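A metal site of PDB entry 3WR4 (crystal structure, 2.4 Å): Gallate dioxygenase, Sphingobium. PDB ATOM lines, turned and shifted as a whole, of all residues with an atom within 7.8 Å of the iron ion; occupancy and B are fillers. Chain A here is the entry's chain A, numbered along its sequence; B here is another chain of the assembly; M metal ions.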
ATOM      1  N   HIS A  12     -22.226  27.713  -4.101  1.00  0.00           N
ATOM      2  CA  HIS A  12     -23.372  27.526  -3.226  1.00  0.00           C
ATOM      3  C   HIS A  12     -23.166  26.352  -2.300  1.00  0.00           C
ATOM      4  O   HIS A  12     -24.116  25.668  -1.907  1.00  0.00           O
ATOM      5  CB  HIS A  12     -24.689  27.398  -4.015  1.00  0.00           C
ATOM      6  CG  HIS A  12     -24.734  26.268  -4.998  1.00  0.00           C
ATOM      7  ND1 HIS A  12     -24.029  26.265  -6.181  1.00  0.00           N
ATOM      8  CD2 HIS A  12     -25.480  25.129  -5.004  1.00  0.00           C
ATOM      9  CE1 HIS A  12     -24.310  25.169  -6.865  1.00  0.00           C
ATOM     10  NE2 HIS A  12     -25.174  24.454  -6.162  1.00  0.00           N
ATOM     11  N   THR A  13     -21.904  26.146  -1.955  1.00  0.00           N
ATOM     12  CA  THR A  13     -21.480  25.313  -0.834  1.00  0.00           C
ATOM     13  C   THR A  13     -22.414  25.440   0.370  1.00  0.00           C
ATOM     14  O   THR A  13     -22.776  26.563   0.756  1.00  0.00           O
ATOM     15  CB  THR A  13     -20.059  25.703  -0.399  1.00  0.00           C
ATOM     16  OG1 THR A  13     -19.114  25.139  -1.310  1.00  0.00           O
ATOM     17  CG2 THR A  13     -19.770  25.201   1.006  1.00  0.00           C
ATOM     18  N   PRO A  14     -22.815  24.306   0.960  1.00  0.00           N
ATOM     19  CA  PRO A  14     -23.740  24.339   2.104  1.00  0.00           C
ATOM     20  C   PRO A  14     -23.128  24.780   3.439  1.00  0.00           C
ATOM     21  O   PRO A  14     -23.892  25.147   4.335  1.00  0.00           O
ATOM     22  CB  PRO A  14     -24.214  22.883   2.203  1.00  0.00           C
ATOM     23  CG  PRO A  14     -23.109  22.083   1.630  1.00  0.00           C
ATOM     24  CD  PRO A  14     -22.496  22.929   0.532  1.00  0.00           C
ATOM     25  N   TYR A  56     -29.142  27.971 -10.154  1.00  0.00           N
ATOM     26  CA  TYR A  56     -28.470  27.073  -9.224  1.00  0.00           C
ATOM     27  C   TYR A  56     -28.673  25.598  -9.594  1.00  0.00           C
ATOM     28  O   TYR A  56     -28.998  25.264 -10.732  1.00  0.00           O
ATOM     29  CB  TYR A  56     -28.975  27.334  -7.820  1.00  0.00           C
ATOM     30  CG  TYR A  56     -30.362  26.824  -7.512  1.00  0.00           C
ATOM     31  CD1 TYR A  56     -30.569  25.896  -6.503  1.00  0.00           C
ATOM     32  CD2 TYR A  56     -31.484  27.281  -8.229  1.00  0.00           C
ATOM     33  CE1 TYR A  56     -31.835  25.434  -6.198  1.00  0.00           C
ATOM     34  CE2 TYR A  56     -32.759  26.806  -7.939  1.00  0.00           C
ATOM     35  CZ  TYR A  56     -32.923  25.893  -6.923  1.00  0.00           C
ATOM     36  OH  TYR A  56     -34.172  25.418  -6.623  1.00  0.00           O
ATOM     37  N   ASN A  57     -28.489  24.698  -8.637  1.00  0.00           N
ATOM     38  CA  ASN A  57     -29.051  23.359  -8.786  1.00  0.00           C
ATOM     39  C   ASN A  57     -29.495  22.804  -7.443  1.00  0.00           C
ATOM     40  O   ASN A  57     -28.821  22.992  -6.422  1.00  0.00           O
ATOM     41  CB  ASN A  57     -28.056  22.416  -9.480  1.00  0.00           C
ATOM     42  CG  ASN A  57     -26.965  21.898  -8.566  1.00  0.00           C
ATOM     43  OD1 ASN A  57     -27.158  20.963  -7.789  1.00  0.00           O
ATOM     44  ND2 ASN A  57     -25.805  22.515  -8.659  1.00  0.00           N
ATOM     45  N   ASP A  58     -30.663  22.187  -7.427  1.00  0.00           N
ATOM     46  CA  ASP A  58     -31.153  21.454  -6.260  1.00  0.00           C
ATOM     47  C   ASP A  58     -30.293  20.222  -6.067  1.00  0.00           C
ATOM     48  O   ASP A  58     -29.900  19.570  -7.038  1.00  0.00           O
ATOM     49  CB  ASP A  58     -32.627  21.054  -6.437  1.00  0.00           C
ATOM     50  CG  ASP A  58     -33.207  20.362  -5.213  1.00  0.00           C
ATOM     51  OD1 ASP A  58     -33.664  21.066  -4.294  1.00  0.00           O
ATOM     52  OD2 ASP A  58     -33.230  19.107  -5.168  1.00  0.00           O
ATOM     53  N   HIS A  59     -30.004  19.911  -4.804  1.00  0.00           N
ATOM     54  CA  HIS A  59     -29.142  18.774  -4.483  1.00  0.00           C
ATOM     55  C   HIS A  59     -29.985  17.634  -3.945  1.00  0.00           C
ATOM     56  O   HIS A  59     -29.845  17.205  -2.784  1.00  0.00           O
ATOM     57  CB  HIS A  59     -28.059  19.186  -3.486  1.00  0.00           C
ATOM     58  CG  HIS A  59     -27.121  20.217  -4.032  1.00  0.00           C
ATOM     59  ND1 HIS A  59     -27.444  21.553  -4.104  1.00  0.00           N
ATOM     60  CD2 HIS A  59     -25.883  20.111  -4.589  1.00  0.00           C
ATOM     61  CE1 HIS A  59     -26.450  22.224  -4.654  1.00  0.00           C
ATOM     62  NE2 HIS A  59     -25.490  21.367  -4.965  1.00  0.00           N
ATOM     63  N   ASP A 123     -33.364  24.806  -1.759  1.00  0.00           N
ATOM     64  CA  ASP A 123     -32.387  24.219  -0.842  1.00  0.00           C
ATOM     65  C   ASP A 123     -31.189  25.166  -0.704  1.00  0.00           C
ATOM     66  O   ASP A 123     -31.248  26.287  -1.203  1.00  0.00           O
ATOM     67  CB  ASP A 123     -31.992  22.806  -1.309  1.00  0.00           C
ATOM     68  CG  ASP A 123     -30.977  22.800  -2.470  1.00  0.00           C
ATOM     69  OD1 ASP A 123     -30.825  23.813  -3.179  1.00  0.00           O
ATOM     70  OD2 ASP A 123     -30.334  21.749  -2.665  1.00  0.00           O
ATOM     71  N   HIS A 124     -30.113  24.719  -0.046  1.00  0.00           N
ATOM     72  CA  HIS A 124     -28.974  25.602   0.224  1.00  0.00           C
ATOM     73  C   HIS A 124     -28.432  26.193  -1.078  1.00  0.00           C
ATOM     74  O   HIS A 124     -27.907  27.295  -1.086  1.00  0.00           O
ATOM     75  CB  HIS A 124     -27.853  24.871   0.988  1.00  0.00           C
ATOM     76  CG  HIS A 124     -27.142  23.820   0.184  1.00  0.00           C
ATOM     77  ND1 HIS A 124     -26.100  24.108  -0.677  1.00  0.00           N
ATOM     78  CD2 HIS A 124     -27.309  22.468   0.132  1.00  0.00           C
ATOM     79  CE1 HIS A 124     -25.674  22.988  -1.232  1.00  0.00           C
ATOM     80  NE2 HIS A 124     -26.387  21.986  -0.758  1.00  0.00           N
ATOM     81  N   GLY A 125     -28.602  25.465  -2.176  1.00  0.00           N
ATOM     82  CA  GLY A 125     -28.104  25.897  -3.479  1.00  0.00           C
ATOM     83  C   GLY A 125     -28.540  27.291  -3.869  1.00  0.00           C
ATOM     84  O   GLY A 125     -27.902  27.970  -4.673  1.00  0.00           O
ATOM     85  N   VAL A 151     -28.073  18.977 -12.973  1.00  0.00           N
ATOM     86  CA  VAL A 151     -26.691  18.700 -13.310  1.00  0.00           C
ATOM     87  C   VAL A 151     -26.157  17.394 -12.744  1.00  0.00           C
ATOM     88  O   VAL A 151     -25.037  16.978 -13.067  1.00  0.00           O
ATOM     89  CB  VAL A 151     -25.798  19.854 -12.837  1.00  0.00           C
ATOM     90  CG1 VAL A 151     -25.982  21.069 -13.741  1.00  0.00           C
ATOM     91  CG2 VAL A 151     -26.123  20.176 -11.390  1.00  0.00           C
ATOM     92  N   LEU A 152     -26.953  16.741 -11.901  1.00  0.00           N
ATOM     93  CA  LEU A 152     -26.508  15.551 -11.164  1.00  0.00           C
ATOM     94  C   LEU A 152     -26.750  14.195 -11.849  1.00  0.00           C
ATOM     95  O   LEU A 152     -26.132  13.206 -11.466  1.00  0.00           O
ATOM     96  CB  LEU A 152     -27.189  15.546  -9.791  1.00  0.00           C
ATOM     97  CG  LEU A 152     -26.974  16.835  -8.994  1.00  0.00           C
ATOM     98  CD1 LEU A 152     -27.632  16.752  -7.619  1.00  0.00           C
ATOM     99  CD2 LEU A 152     -25.476  17.099  -8.876  1.00  0.00           C
ATOM    100  N   THR A 187     -24.850  30.788  -9.883  1.00  0.00           N
ATOM    101  CA  THR A 187     -24.488  30.025  -8.703  1.00  0.00           C
ATOM    102  C   THR A 187     -23.759  28.723  -9.074  1.00  0.00           C
ATOM    103  O   THR A 187     -23.908  28.239 -10.193  1.00  0.00           O
ATOM    104  CB  THR A 187     -25.780  29.779  -7.880  1.00  0.00           C
ATOM    105  OG1 THR A 187     -25.966  30.878  -6.966  1.00  0.00           O
ATOM    106  CG2 THR A 187     -25.780  28.513  -7.128  1.00  0.00           C
ATOM    107  N   GLY A 188     -22.920  28.205  -8.192  1.00  0.00           N
ATOM    108  CA  GLY A 188     -22.230  26.959  -8.485  1.00  0.00           C
ATOM    109  C   GLY A 188     -20.737  26.976  -8.309  1.00  0.00           C
ATOM    110  O   GLY A 188     -20.121  28.045  -8.296  1.00  0.00           O
ATOM    111  N   GLY A 189     -20.158  25.781  -8.177  1.00  0.00           N
ATOM    112  CA  GLY A 189     -18.711  25.572  -8.192  1.00  0.00           C
ATOM    113  C   GLY A 189     -17.974  25.909  -6.905  1.00  0.00           C
ATOM    114  O   GLY A 189     -18.587  26.148  -5.868  1.00  0.00           O
ATOM    115  N   HIS A 192     -14.397  20.807  -7.004  1.00  0.00           N
ATOM    116  CA  HIS A 192     -14.418  19.951  -5.830  1.00  0.00           C
ATOM    117  C   HIS A 192     -14.768  18.522  -6.231  1.00  0.00           C
ATOM    118  O   HIS A 192     -14.865  18.202  -7.409  1.00  0.00           O
ATOM    119  CB  HIS A 192     -15.373  20.487  -4.775  1.00  0.00           C
ATOM    120  CG  HIS A 192     -16.799  20.589  -5.226  1.00  0.00           C
ATOM    121  ND1 HIS A 192     -17.167  21.222  -6.389  1.00  0.00           N
ATOM    122  CD2 HIS A 192     -17.940  20.151  -4.655  1.00  0.00           C
ATOM    123  CE1 HIS A 192     -18.486  21.159  -6.526  1.00  0.00           C
ATOM    124  NE2 HIS A 192     -18.972  20.523  -5.487  1.00  0.00           N
ATOM    125  N   GLU A 236     -18.451  16.725  -9.186  1.00  0.00           N
ATOM    126  CA  GLU A 236     -19.413  17.754  -8.815  1.00  0.00           C
ATOM    127  C   GLU A 236     -18.987  19.153  -9.260  1.00  0.00           C
ATOM    128  O   GLU A 236     -19.794  20.071  -9.325  1.00  0.00           O
ATOM    129  CB  GLU A 236     -19.663  17.740  -7.298  1.00  0.00           C
ATOM    130  CG  GLU A 236     -20.487  16.567  -6.788  1.00  0.00           C
ATOM    131  CD  GLU A 236     -19.670  15.288  -6.563  1.00  0.00           C
ATOM    132  OE1 GLU A 236     -18.535  15.161  -7.088  1.00  0.00           O
ATOM    133  OE2 GLU A 236     -20.184  14.409  -5.840  1.00  0.00           O
ATOM    134  N   GLY A 237     -17.702  19.304  -9.569  1.00  0.00           N
ATOM    135  CA  GLY A 237     -17.150  20.567 -10.023  1.00  0.00           C
ATOM    136  C   GLY A 237     -17.669  20.874 -11.418  1.00  0.00           C
ATOM    137  O   GLY A 237     -17.748  22.037 -11.845  1.00  0.00           O
ATOM    138  N   GLU A 239     -20.397  21.034 -12.503  1.00  0.00           N
ATOM    139  CA  GLU A 239     -21.620  21.835 -12.492  1.00  0.00           C
ATOM    140  C   GLU A 239     -21.423  23.265 -12.990  1.00  0.00           C
ATOM    141  O   GLU A 239     -22.391  23.950 -13.324  1.00  0.00           O
ATOM    142  CB  GLU A 239     -22.219  21.887 -11.092  1.00  0.00           C
ATOM    143  CG  GLU A 239     -21.488  22.777 -10.116  1.00  0.00           C
ATOM    144  CD  GLU A 239     -22.090  22.652  -8.725  1.00  0.00           C
ATOM    145  OE1 GLU A 239     -23.218  22.128  -8.620  1.00  0.00           O
ATOM    146  OE2 GLU A 239     -21.433  23.041  -7.744  1.00  0.00           O
ATOM    147  N   VAL A 240     -20.167  23.722 -13.074  1.00  0.00           N
ATOM    148  CA  VAL A 240     -19.917  25.092 -13.515  1.00  0.00           C
ATOM    149  C   VAL A 240     -20.399  25.424 -14.946  1.00  0.00           C
ATOM    150  O   VAL A 240     -20.202  26.552 -15.400  1.00  0.00           O
ATOM    151  CB  VAL A 240     -18.403  25.440 -13.457  1.00  0.00           C
ATOM    152  CG1 VAL A 240     -17.862  25.218 -12.045  1.00  0.00           C
ATOM    153  CG2 VAL A 240     -17.638  24.623 -14.485  1.00  0.00           C
ATOM    154  N   MET A 242     -23.302  25.757 -15.403  1.00  0.00           N
ATOM    155  CA  MET A 242     -24.222  26.757 -14.921  1.00  0.00           C
ATOM    156  C   MET A 242     -23.632  28.168 -15.023  1.00  0.00           C
ATOM    157  O   MET A 242     -24.336  29.086 -15.457  1.00  0.00           O
ATOM    158  CB  MET A 242     -24.644  26.431 -13.503  1.00  0.00           C
ATOM    159  CG  MET A 242     -25.557  25.222 -13.429  1.00  0.00           C
ATOM    160  SD  MET A 242     -26.210  25.002 -11.787  1.00  0.00           S
ATOM    161  CE  MET A 242     -24.720  24.499 -10.944  1.00  0.00           C
ATOM    162  N   PHE B 374     -25.597  13.273  -2.128  1.00  0.00           N
ATOM    163  CA  PHE B 374     -26.504  14.231  -1.484  1.00  0.00           C
ATOM    164  C   PHE B 374     -27.605  13.593  -0.638  1.00  0.00           C
ATOM    165  O   PHE B 374     -28.166  14.240   0.235  1.00  0.00           O
ATOM    166  CB  PHE B 374     -27.095  15.130  -2.544  1.00  0.00           C
ATOM    167  CG  PHE B 374     -26.066  15.844  -3.323  1.00  0.00           C
ATOM    168  CD1 PHE B 374     -25.242  16.783  -2.706  1.00  0.00           C
ATOM    169  CD2 PHE B 374     -25.876  15.563  -4.657  1.00  0.00           C
ATOM    170  CE1 PHE B 374     -24.263  17.453  -3.412  1.00  0.00           C
ATOM    171  CE2 PHE B 374     -24.897  16.242  -5.384  1.00  0.00           C
ATOM    172  CZ  PHE B 374     -24.090  17.180  -4.762  1.00  0.00           C
HETATM  173 FE    FE M   1     -24.138  21.938  -6.798  1.00  0.00          FE
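The side-chain carboxylate (OE2) of Glu 239 sits at hydrogen-bond distance from the backbone NH (N) of Gly 189, at 3.1 Å. A ring nitrogen (NE2) of His 59 lies close to a ring nitrogen (NE2) of His 12 (3.3 Å). The side-chain carboxylate (OD2) of Asp 123 is in hydrogen-bond range of the backbone NH (N) of His 59, 2.8 Å away. The side-chain amide nitrogen (ND2) of Asn 57 lies close to a ring nitrogen (NE2) of His 12 (3.2 Å). ND1 of His 12 sits close to N of Gly 188 (3.0 Å). A ring nitrogen (ND1) of His 124 sits at hydrogen-bond distance from the backbone carbonyl oxygen of His 12, 2.8 Å away.
Within 4 Å of the iron ion: His 12, Asn 57, His 59 and Glu 239. The nearest printed residue that does not touch the iron ion is Met 242 (4.9 Å).
The iron ion is bound by OE1 of Glu 239 (2.0 Å), NE2 of His 59 (2.3 Å) and ND2 of Asn 57 (2.6 Å). The iron ion has three donor atoms within binding distance. Slightly farther from the iron ion lies a ring nitrogen (NE2) of His 12 (2.8 Å).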
